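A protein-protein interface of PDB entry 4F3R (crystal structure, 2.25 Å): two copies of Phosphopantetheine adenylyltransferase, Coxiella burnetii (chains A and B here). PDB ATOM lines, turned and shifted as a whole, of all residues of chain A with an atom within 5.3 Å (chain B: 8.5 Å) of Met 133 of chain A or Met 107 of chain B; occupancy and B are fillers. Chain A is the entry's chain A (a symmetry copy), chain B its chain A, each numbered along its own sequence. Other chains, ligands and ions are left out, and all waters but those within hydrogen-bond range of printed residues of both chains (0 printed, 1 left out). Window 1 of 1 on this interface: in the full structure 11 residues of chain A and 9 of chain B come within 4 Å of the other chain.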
ATOM      1  N   TYR A 128     -18.147  -1.706  12.718  1.00  0.00           N
ATOM      2  CA  TYR A 128     -19.084  -0.800  12.045  1.00  0.00           C
ATOM      3  C   TYR A 128     -19.138  -1.009  10.529  1.00  0.00           C
ATOM      4  O   TYR A 128     -20.047  -0.510   9.862  1.00  0.00           O
ATOM      5  CB  TYR A 128     -18.712   0.658  12.341  1.00  0.00           C
ATOM      6  CG  TYR A 128     -17.331   1.059  11.855  1.00  0.00           C
ATOM      7  CD1 TYR A 128     -16.212   0.946  12.685  1.00  0.00           C
ATOM      8  CD2 TYR A 128     -17.143   1.547  10.562  1.00  0.00           C
ATOM      9  CE1 TYR A 128     -14.940   1.311  12.241  1.00  0.00           C
ATOM     10  CE2 TYR A 128     -15.874   1.914  10.108  1.00  0.00           C
ATOM     11  CZ  TYR A 128     -14.776   1.794  10.950  1.00  0.00           C
ATOM     12  OH  TYR A 128     -13.526   2.156  10.494  1.00  0.00           O
ATOM     13  N   VAL A 129     -18.161  -1.727   9.987  1.00  0.00           N
ATOM     14  CA  VAL A 129     -18.033  -1.891   8.554  1.00  0.00           C
ATOM     15  C   VAL A 129     -18.888  -3.042   8.049  1.00  0.00           C
ATOM     16  O   VAL A 129     -18.444  -4.199   8.047  1.00  0.00           O
ATOM     17  CB  VAL A 129     -16.569  -2.156   8.162  1.00  0.00           C
ATOM     18  CG1 VAL A 129     -16.468  -2.548   6.694  1.00  0.00           C
ATOM     19  CG2 VAL A 129     -15.723  -0.929   8.463  1.00  0.00           C
ATOM     20  N   SER A 130     -20.097  -2.710   7.601  1.00  0.00           N
ATOM     21  CA  SER A 130     -21.050  -3.686   7.078  1.00  0.00           C
ATOM     22  C   SER A 130     -21.276  -3.519   5.575  1.00  0.00           C
ATOM     23  O   SER A 130     -21.136  -2.419   5.029  1.00  0.00           O
ATOM     24  CB  SER A 130     -22.388  -3.541   7.803  1.00  0.00           C
ATOM     25  OG  SER A 130     -22.962  -2.265   7.585  1.00  0.00           O
ATOM     26  N   GLY A 131     -21.665  -4.610   4.923  1.00  0.00           N
ATOM     27  CA  GLY A 131     -21.902  -4.627   3.482  1.00  0.00           C
ATOM     28  C   GLY A 131     -22.878  -3.583   2.992  1.00  0.00           C
ATOM     29  O   GLY A 131     -22.586  -2.859   2.039  1.00  0.00           O
ATOM     30  N   THR A 132     -24.040  -3.497   3.639  1.00  0.00           N
ATOM     31  CA  THR A 132     -25.063  -2.531   3.241  1.00  0.00           C
ATOM     32  C   THR A 132     -24.612  -1.092   3.510  1.00  0.00           C
ATOM     33  O   THR A 132     -25.006  -0.170   2.798  1.00  0.00           O
ATOM     34  CB  THR A 132     -26.436  -2.808   3.921  1.00  0.00           C
ATOM     35  OG1 THR A 132     -27.234  -1.621   3.890  1.00  0.00           O
ATOM     36  CG2 THR A 132     -26.273  -3.248   5.364  1.00  0.00           C
ATOM     37  N   MET A 133     -23.780  -0.923   4.538  1.00  0.00           N
ATOM     38  CA  MET A 133     -23.175   0.369   4.888  1.00  0.00           C
ATOM     39  C   MET A 133     -22.217   0.782   3.767  1.00  0.00           C
ATOM     40  O   MET A 133     -22.400   1.814   3.127  1.00  0.00           O
ATOM     41  CB  MET A 133     -22.443   0.222   6.234  1.00  0.00           C
ATOM     42  CG  MET A 133     -21.800   1.456   6.832  1.00  0.00           C
ATOM     43  SD  MET A 133     -22.917   2.232   8.237  1.00  0.00           S
ATOM     44  CE  MET A 133     -23.962   3.384   7.051  1.00  0.00           C
ATOM     45  N   VAL A 134     -21.228  -0.069   3.505  1.00  0.00           N
ATOM     46  CA  VAL A 134     -20.253   0.159   2.433  1.00  0.00           C
ATOM     47  C   VAL A 134     -20.912   0.351   1.062  1.00  0.00           C
ATOM     48  O   VAL A 134     -20.517   1.218   0.292  1.00  0.00           O
ATOM     49  CB  VAL A 134     -19.246  -1.001   2.366  1.00  0.00           C
ATOM     50  CG1 VAL A 134     -18.350  -0.873   1.141  1.00  0.00           C
ATOM     51  CG2 VAL A 134     -18.419  -1.046   3.636  1.00  0.00           C
ATOM     52  N   ARG A 135     -21.921  -0.456   0.770  1.00  0.00           N
ATOM     53  CA  ARG A 135     -22.675  -0.337  -0.480  1.00  0.00           C
ATOM     54  C   ARG A 135     -23.402   1.012  -0.589  1.00  0.00           C
ATOM     55  O   ARG A 135     -23.476   1.595  -1.674  1.00  0.00           O
ATOM     56  CB  ARG A 135     -23.664  -1.503  -0.595  1.00  0.00           C
ATOM     57  CG  ARG A 135     -24.073  -1.887  -1.994  1.00  0.00           C
ATOM     58  CD  ARG A 135     -24.559  -3.347  -2.021  1.00  0.00           C
ATOM     59  NE  ARG A 135     -25.636  -3.610  -1.054  1.00  0.00           N
ATOM     60  CZ  ARG A 135     -25.595  -4.479  -0.042  1.00  0.00           C
ATOM     61  NH1 ARG A 135     -24.530  -5.238   0.196  1.00  0.00           N
ATOM     62  NH2 ARG A 135     -26.655  -4.599   0.750  1.00  0.00           N
ATOM     63  N   GLU A 136     -23.927   1.514   0.531  1.00  0.00           N
ATOM     64  CA  GLU A 136     -24.559   2.840   0.541  1.00  0.00           C
ATOM     65  C   GLU A 136     -23.531   3.903   0.159  1.00  0.00           C
ATOM     66  O   GLU A 136     -23.833   4.805  -0.623  1.00  0.00           O
ATOM     67  CB  GLU A 136     -25.187   3.166   1.909  1.00  0.00           C
ATOM     68  CG  GLU A 136     -26.070   4.437   1.904  1.00  0.00           C
ATOM     69  CD  GLU A 136     -26.596   4.846   3.294  1.00  0.00           C
ATOM     70  OE1 GLU A 136     -26.391   4.099   4.287  1.00  0.00           O
ATOM     71  OE2 GLU A 136     -27.219   5.932   3.386  1.00  0.00           O
ATOM     72  N   ILE A 137     -22.314   3.770   0.692  1.00  0.00           N
ATOM     73  CA  ILE A 137     -21.213   4.698   0.395  1.00  0.00           C
ATOM     74  C   ILE A 137     -20.850   4.698  -1.087  1.00  0.00           C
ATOM     75  O   ILE A 137     -20.724   5.767  -1.697  1.00  0.00           O
ATOM     76  CB  ILE A 137     -19.927   4.371   1.202  1.00  0.00           C
ATOM     77  CG1 ILE A 137     -20.176   4.448   2.715  1.00  0.00           C
ATOM     78  CG2 ILE A 137     -18.797   5.315   0.816  1.00  0.00           C
ATOM     79  CD1 ILE A 137     -20.677   5.792   3.182  1.00  0.00           C
ATOM     80  N   PHE A 147     -11.932   0.243   3.520  1.00  0.00           N
ATOM     81  CA  PHE A 147     -12.782  -0.780   4.110  1.00  0.00           C
ATOM     82  C   PHE A 147     -12.745  -2.120   3.397  1.00  0.00           C
ATOM     83  O   PHE A 147     -13.209  -3.128   3.945  1.00  0.00           O
ATOM     84  CB  PHE A 147     -14.210  -0.269   4.116  1.00  0.00           C
ATOM     85  CG  PHE A 147     -14.334   1.106   4.660  1.00  0.00           C
ATOM     86  CD1 PHE A 147     -14.118   1.341   6.002  1.00  0.00           C
ATOM     87  CD2 PHE A 147     -14.636   2.170   3.835  1.00  0.00           C
ATOM     88  CE1 PHE A 147     -14.215   2.600   6.509  1.00  0.00           C
ATOM     89  CE2 PHE A 147     -14.740   3.446   4.345  1.00  0.00           C
ATOM     90  CZ  PHE A 147     -14.524   3.662   5.680  1.00  0.00           C
ATOM     91  N   LEU B  75     -22.792  12.154   0.124  1.00  0.00           N
ATOM     92  CA  LEU B  75     -22.473  11.725   1.478  1.00  0.00           C
ATOM     93  C   LEU B  75     -22.831  12.809   2.475  1.00  0.00           C
ATOM     94  O   LEU B  75     -22.676  13.993   2.204  1.00  0.00           O
ATOM     95  CB  LEU B  75     -20.984  11.418   1.640  1.00  0.00           C
ATOM     96  CG  LEU B  75     -20.403  10.146   1.041  1.00  0.00           C
ATOM     97  CD1 LEU B  75     -18.917  10.100   1.356  1.00  0.00           C
ATOM     98  CD2 LEU B  75     -21.110   8.920   1.585  1.00  0.00           C
ATOM     99  N   VAL B  77     -21.307  13.432   5.310  1.00  0.00           N
ATOM    100  CA  VAL B  77     -20.115  14.121   5.818  1.00  0.00           C
ATOM    101  C   VAL B  77     -19.617  15.158   4.821  1.00  0.00           C
ATOM    102  O   VAL B  77     -19.070  16.175   5.221  1.00  0.00           O
ATOM    103  CB  VAL B  77     -18.961  13.158   6.206  1.00  0.00           C
ATOM    104  CG1 VAL B  77     -19.406  12.235   7.316  1.00  0.00           C
ATOM    105  CG2 VAL B  77     -18.451  12.382   4.993  1.00  0.00           C
ATOM    106  N   ILE B  88     -23.258  16.299  13.560  1.00  0.00           N
ATOM    107  CA  ILE B  88     -24.424  15.604  13.056  1.00  0.00           C
ATOM    108  C   ILE B  88     -25.344  15.351  14.252  1.00  0.00           C
ATOM    109  O   ILE B  88     -24.930  14.763  15.244  1.00  0.00           O
ATOM    110  CB  ILE B  88     -24.024  14.266  12.410  1.00  0.00           C
ATOM    111  CG1 ILE B  88     -23.096  14.514  11.225  1.00  0.00           C
ATOM    112  CG2 ILE B  88     -25.264  13.484  11.944  1.00  0.00           C
ATOM    113  CD1 ILE B  88     -22.354  13.277  10.777  1.00  0.00           C
ATOM    114  N   ASP B  99     -28.138   0.781  17.909  1.00  0.00           N
ATOM    115  CA  ASP B  99     -27.156  -0.097  17.280  1.00  0.00           C
ATOM    116  C   ASP B  99     -26.771   0.424  15.895  1.00  0.00           C
ATOM    117  O   ASP B  99     -25.598   0.495  15.558  1.00  0.00           O
ATOM    118  CB  ASP B  99     -27.667  -1.550  17.208  1.00  0.00           C
ATOM    119  CG  ASP B  99     -26.586  -2.568  17.557  1.00  0.00           C
ATOM    120  OD1 ASP B  99     -25.379  -2.222  17.499  1.00  0.00           O
ATOM    121  OD2 ASP B  99     -26.946  -3.710  17.915  1.00  0.00           O
ATOM    122  N   TYR B 100     -27.765   0.803  15.106  1.00  0.00           N
ATOM    123  CA  TYR B 100     -27.530   1.312  13.758  1.00  0.00           C
ATOM    124  C   TYR B 100     -26.870   2.699  13.744  1.00  0.00           C
ATOM    125  O   TYR B 100     -25.992   2.963  12.931  1.00  0.00           O
ATOM    126  CB  TYR B 100     -28.855   1.360  12.985  1.00  0.00           C
ATOM    127  CG  TYR B 100     -28.770   2.107  11.682  1.00  0.00           C
ATOM    128  CD1 TYR B 100     -28.265   1.491  10.542  1.00  0.00           C
ATOM    129  CD2 TYR B 100     -29.191   3.419  11.584  1.00  0.00           C
ATOM    130  CE1 TYR B 100     -28.189   2.169   9.325  1.00  0.00           C
ATOM    131  CE2 TYR B 100     -29.110   4.111  10.380  1.00  0.00           C
ATOM    132  CZ  TYR B 100     -28.608   3.471   9.253  1.00  0.00           C
ATOM    133  OH  TYR B 100     -28.526   4.142   8.057  1.00  0.00           O
ATOM    134  N   GLU B 101     -27.305   3.587  14.631  1.00  0.00           N
ATOM    135  CA  GLU B 101     -26.721   4.913  14.711  1.00  0.00           C
ATOM    136  C   GLU B 101     -25.279   4.880  15.214  1.00  0.00           C
ATOM    137  O   GLU B 101     -24.464   5.707  14.824  1.00  0.00           O
ATOM    138  CB  GLU B 101     -27.561   5.819  15.614  1.00  0.00           C
ATOM    139  CG  GLU B 101     -28.980   6.082  15.109  1.00  0.00           C
ATOM    140  CD  GLU B 101     -29.012   6.819  13.803  1.00  0.00           C
ATOM    141  OE1 GLU B 101     -28.041   7.544  13.484  1.00  0.00           O
ATOM    142  OE2 GLU B 101     -30.016   6.677  13.069  1.00  0.00           O
ATOM    143  N   PHE B 102     -24.986   3.925  16.087  1.00  0.00           N
ATOM    144  CA  PHE B 102     -23.653   3.760  16.655  1.00  0.00           C
ATOM    145  C   PHE B 102     -22.707   3.357  15.534  1.00  0.00           C
ATOM    146  O   PHE B 102     -21.600   3.868  15.432  1.00  0.00           O
ATOM    147  CB  PHE B 102     -23.702   2.697  17.765  1.00  0.00           C
ATOM    148  CG  PHE B 102     -22.522   2.692  18.692  1.00  0.00           C
ATOM    149  CD1 PHE B 102     -22.151   3.829  19.378  1.00  0.00           C
ATOM    150  CD2 PHE B 102     -21.824   1.512  18.932  1.00  0.00           C
ATOM    151  CE1 PHE B 102     -21.066   3.816  20.255  1.00  0.00           C
ATOM    152  CE2 PHE B 102     -20.738   1.476  19.818  1.00  0.00           C
ATOM    153  CZ  PHE B 102     -20.359   2.641  20.478  1.00  0.00           C
ATOM    154  N   GLN B 103     -23.175   2.458  14.670  1.00  0.00           N
ATOM    155  CA  GLN B 103     -22.389   1.979  13.540  1.00  0.00           C
ATOM    156  C   GLN B 103     -22.190   3.082  12.507  1.00  0.00           C
ATOM    157  O   GLN B 103     -21.090   3.256  11.985  1.00  0.00           O
ATOM    158  CB  GLN B 103     -23.053   0.739  12.907  1.00  0.00           C
ATOM    159  CG  GLN B 103     -23.045  -0.494  13.828  1.00  0.00           C
ATOM    160  CD  GLN B 103     -23.979  -1.621  13.363  1.00  0.00           C
ATOM    161  OE1 GLN B 103     -24.137  -1.867  12.154  1.00  0.00           O
ATOM    162  NE2 GLN B 103     -24.593  -2.318  14.324  1.00  0.00           N
ATOM    163  N   LEU B 104     -23.249   3.825  12.222  1.00  0.00           N
ATOM    164  CA  LEU B 104     -23.173   4.953  11.304  1.00  0.00           C
ATOM    165  C   LEU B 104     -22.260   6.094  11.819  1.00  0.00           C
ATOM    166  O   LEU B 104     -21.534   6.729  11.036  1.00  0.00           O
ATOM    167  CB  LEU B 104     -24.578   5.509  11.047  1.00  0.00           C
ATOM    168  CG  LEU B 104     -24.704   6.540   9.923  1.00  0.00           C
ATOM    169  CD1 LEU B 104     -24.416   5.857   8.578  1.00  0.00           C
ATOM    170  CD2 LEU B 104     -26.082   7.204   9.905  1.00  0.00           C
ATOM    171  N   ALA B 105     -22.326   6.382  13.116  1.00  0.00           N
ATOM    172  CA  ALA B 105     -21.468   7.409  13.701  1.00  0.00           C
ATOM    173  C   ALA B 105     -20.007   7.019  13.481  1.00  0.00           C
ATOM    174  O   ALA B 105     -19.208   7.840  13.071  1.00  0.00           O
ATOM    175  CB  ALA B 105     -21.754   7.588  15.206  1.00  0.00           C
ATOM    176  N   HIS B 106     -19.680   5.762  13.760  1.00  0.00           N
ATOM    177  CA  HIS B 106     -18.327   5.251  13.561  1.00  0.00           C
ATOM    178  C   HIS B 106     -17.891   5.342  12.100  1.00  0.00           C
ATOM    179  O   HIS B 106     -16.788   5.789  11.797  1.00  0.00           O
ATOM    180  CB  HIS B 106     -18.220   3.793  14.006  1.00  0.00           C
ATOM    181  CG  HIS B 106     -18.257   3.601  15.488  1.00  0.00           C
ATOM    182  ND1 HIS B 106     -18.166   4.647  16.383  1.00  0.00           N
ATOM    183  CD2 HIS B 106     -18.347   2.474  16.235  1.00  0.00           C
ATOM    184  CE1 HIS B 106     -18.212   4.172  17.615  1.00  0.00           C
ATOM    185  NE2 HIS B 106     -18.317   2.858  17.556  1.00  0.00           N
ATOM    186  N   MET B 107     -18.762   4.903  11.200  1.00  0.00           N
ATOM    187  CA  MET B 107     -18.469   4.949   9.769  1.00  0.00           C
ATOM    188  C   MET B 107     -18.173   6.384   9.343  1.00  0.00           C
ATOM    189  O   MET B 107     -17.183   6.644   8.666  1.00  0.00           O
ATOM    190  CB  MET B 107     -19.637   4.378   8.945  1.00  0.00           C
ATOM    191  CG  MET B 107     -19.457   4.516   7.450  1.00  0.00           C
ATOM    192  SD  MET B 107     -17.694   3.859   6.868  1.00  0.00           S
ATOM    193  CE  MET B 107     -18.063   1.972   6.469  1.00  0.00           C
ATOM    194  N   ASN B 108     -19.025   7.309   9.764  1.00  0.00           N
ATOM    195  CA  ASN B 108     -18.850   8.721   9.417  1.00  0.00           C
ATOM    196  C   ASN B 108     -17.615   9.340  10.049  1.00  0.00           C
ATOM    197  O   ASN B 108     -17.047  10.280   9.498  1.00  0.00           O
ATOM    198  CB  ASN B 108     -20.084   9.526   9.799  1.00  0.00           C
ATOM    199  CG  ASN B 108     -21.230   9.326   8.837  1.00  0.00           C
ATOM    200  OD1 ASN B 108     -21.032   8.950   7.686  1.00  0.00           O
ATOM    201  ND2 ASN B 108     -22.433   9.576   9.302  1.00  0.00           N
ATOM    202  N   TYR B 109     -17.207   8.820  11.203  1.00  0.00           N
ATOM    203  CA  TYR B 109     -15.985   9.267  11.844  1.00  0.00           C
ATOM    204  C   TYR B 109     -14.783   8.858  11.004  1.00  0.00           C
ATOM    205  O   TYR B 109     -13.890   9.662  10.787  1.00  0.00           O
ATOM    206  CB  TYR B 109     -15.844   8.715  13.266  1.00  0.00           C
ATOM    207  CG  TYR B 109     -14.521   9.094  13.893  1.00  0.00           C
ATOM    208  CD1 TYR B 109     -14.269  10.399  14.301  1.00  0.00           C
ATOM    209  CD2 TYR B 109     -13.509   8.158  14.048  1.00  0.00           C
ATOM    210  CE1 TYR B 109     -13.041  10.759  14.862  1.00  0.00           C
ATOM    211  CE2 TYR B 109     -12.287   8.505  14.613  1.00  0.00           C
ATOM    212  CZ  TYR B 109     -12.063   9.810  15.018  1.00  0.00           C
ATOM    213  OH  TYR B 109     -10.847  10.152  15.577  1.00  0.00           O
ATOM    214  N   GLN B 110     -14.762   7.613  10.530  1.00  0.00           N
ATOM    215  CA  GLN B 110     -13.681   7.165   9.659  1.00  0.00           C
ATOM    216  C   GLN B 110     -13.708   7.940   8.335  1.00  0.00           C
ATOM    217  O   GLN B 110     -12.667   8.339   7.839  1.00  0.00           O
ATOM    218  CB  GLN B 110     -13.732   5.648   9.428  1.00  0.00           C
ATOM    219  CG  GLN B 110     -12.648   5.126   8.473  1.00  0.00           C
ATOM    220  CD  GLN B 110     -11.484   4.420   9.152  1.00  0.00           C
ATOM    221  OE1 GLN B 110     -11.203   4.641  10.339  1.00  0.00           O
ATOM    222  NE2 GLN B 110     -10.783   3.566   8.387  1.00  0.00           N
ATOM    223  N   LEU B 111     -14.889   8.173   7.776  1.00  0.00           N
ATOM    224  CA  LEU B 111     -15.000   8.954   6.545  1.00  0.00           C
ATOM    225  C   LEU B 111     -14.532  10.395   6.717  1.00  0.00           C
ATOM    226  O   LEU B 111     -13.956  10.968   5.805  1.00  0.00           O
ATOM    227  CB  LEU B 111     -16.435   8.951   6.015  1.00  0.00           C
ATOM    228  CG  LEU B 111     -16.924   7.620   5.433  1.00  0.00           C
ATOM    229  CD1 LEU B 111     -18.384   7.745   5.040  1.00  0.00           C
ATOM    230  CD2 LEU B 111     -16.064   7.164   4.253  1.00  0.00           C
ATOM    231  N   SER B 112     -14.790  10.980   7.879  1.00  0.00           N
ATOM    232  CA  SER B 112     -14.419  12.356   8.131  1.00  0.00           C
ATOM    233  C   SER B 112     -14.318  12.633   9.636  1.00  0.00           C
ATOM    234  O   SER B 112     -15.306  13.013  10.261  1.00  0.00           O
ATOM    235  CB  SER B 112     -15.431  13.284   7.480  1.00  0.00           C
ATOM    236  OG  SER B 112     -15.130  14.636   7.774  1.00  0.00           O
ATOM    237  N   PRO B 113     -13.112  12.457  10.214  1.00  0.00           N
ATOM    238  CA  PRO B 113     -12.926  12.568  11.667  1.00  0.00           C
ATOM    239  C   PRO B 113     -13.175  13.963  12.265  1.00  0.00           C
ATOM    240  O   PRO B 113     -13.301  14.080  13.477  1.00  0.00           O
ATOM    241  CB  PRO B 113     -11.479  12.130  11.876  1.00  0.00           C
ATOM    242  CG  PRO B 113     -10.815  12.317  10.571  1.00  0.00           C
ATOM    243  CD  PRO B 113     -11.859  12.113   9.524  1.00  0.00           C
ATOM    244  N   ILE B 115     -15.914  15.656  11.802  1.00  0.00           N
ATOM    245  CA  ILE B 115     -17.335  15.739  12.154  1.00  0.00           C
ATOM    246  C   ILE B 115     -17.645  14.852  13.370  1.00  0.00           C
ATOM    247  O   ILE B 115     -17.206  13.698  13.447  1.00  0.00           O
ATOM    248  CB  ILE B 115     -18.274  15.321  10.993  1.00  0.00           C
ATOM    249  CG1 ILE B 115     -17.888  15.962   9.662  1.00  0.00           C
ATOM    250  CG2 ILE B 115     -19.705  15.702  11.318  1.00  0.00           C
ATOM    251  CD1 ILE B 115     -17.937  17.449   9.653  1.00  0.00           C
ATOM    252  N   THR B 117     -20.710  13.202  15.954  1.00  0.00           N
ATOM    253  CA  THR B 117     -22.130  12.859  16.029  1.00  0.00           C
ATOM    254  C   THR B 117     -22.612  12.984  17.467  1.00  0.00           C
ATOM    255  O   THR B 117     -21.970  12.480  18.376  1.00  0.00           O
ATOM    256  CB  THR B 117     -22.419  11.429  15.534  1.00  0.00           C
ATOM    257  OG1 THR B 117     -22.044  11.305  14.161  1.00  0.00           O
ATOM    258  CG2 THR B 117     -23.907  11.110  15.648  1.00  0.00           C
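OE1 of Gln 110 of chain B sits close to OH of Tyr 128 of chain A (3.4 Å).
The backbone carbonyl oxygen of Asp 99 of chain B is in hydrogen-bond range of the side-chain amide nitrogen of Gln 103 of chain B (3.2 Å).
O of Leu 104 of chain B sits close to ND2 of Asn 108 of chain B (3.5 Å).
The backbone NH of Met 133 of chain A lies close to the side-chain hydroxyl of Ser 130 of chain A, at 3.4 Å.
Among the printed residues, pairs that only touch across the chains: Tyr 128 of chain A with Gln 103 of chain B (3.5 Å), Tyr 128 of chain A with His 106 of chain B (3.6 Å), Tyr 128 of chain A with Met 107 of chain B (3.7 Å), Met 133 of chain A with Leu 104 of chain B (2.9 Å), Met 133 of chain A with Met 107 of chain B (3.8 Å), Ile 137 of chain A with Leu 75 of chain B (3.5 Å), Ile 137 of chain A with Leu 111 of chain B (3.5 Å), Phe 147 of chain A with Met 107 of chain B (3.4 Å), Phe 147 of chain A with Gln 110 of chain B (3.6 Å) and Phe 147 of chain A with Leu 111 of chain B (3.9 Å).
Of the printed residues of chain B, Tyr 128 of chain A touches Gln 103 (3.5 Å), His 106 (3.6 Å), Met 107 (3.7 Å) and Gln 110 (3.3 Å).
Ser 130 of chain A touches none of the printed residues of chain B.
No residue of chain B comes within 4 Å of Gly 131 of chain A.
Met 133 of chain A touches just these residues of chain B: Leu 104 (2.9 Å) and Met 107 (3.8 Å).
Printed residues of chain B within 4 Å of Ile 137 of chain A: Leu 75 and Leu 111.
Of the printed residues of chain A, His 106 of chain B touches Tyr 128.
Of chain A, only Tyr 128, Met 133 and Phe 147 come within 4 Å of Met 107 of chain B.
Tyr 109 of chain B touches none of the printed residues of chain A.
Of the printed residues of chain A, Gln 110 of chain B touches Tyr 128 and Phe 147.
Of the printed residues of chain A, Leu 111 of chain B touches Ile 137 (3.5 Å) and Phe 147 (3.9 Å).
Ile 115 of chain B touches none of the printed residues of chain A.
The nearest printed residue of chain A that does not touch Gln 110 of chain B is Val 129 of chain A (6.7 Å).
Of the 11 printed residues of chain A, 4 touch a printed residue of chain B.
Hydrophobic or aromatic side chains of chain A within 4 Å of the printed part of chain B: Tyr 128, Met 133, Ile 137 and Phe 147.
Of the 20 printed residues of chain B, 7 touch a printed residue of chain A.
Along chain B the printed residues that touch a printed residue of chain A span positions 75 to 111.
Among the printed residues, 11 pairs touch across the chains.
Among the printed residues, no Asp or Glu carboxylate lies within 4 Å of a Lys or Arg side-chain nitrogen of the other chain.
No position is printed for both chains.
Of the 11 pairs that touch across the chains among the printed residues, none has its exchanged pair printed and touching as well.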
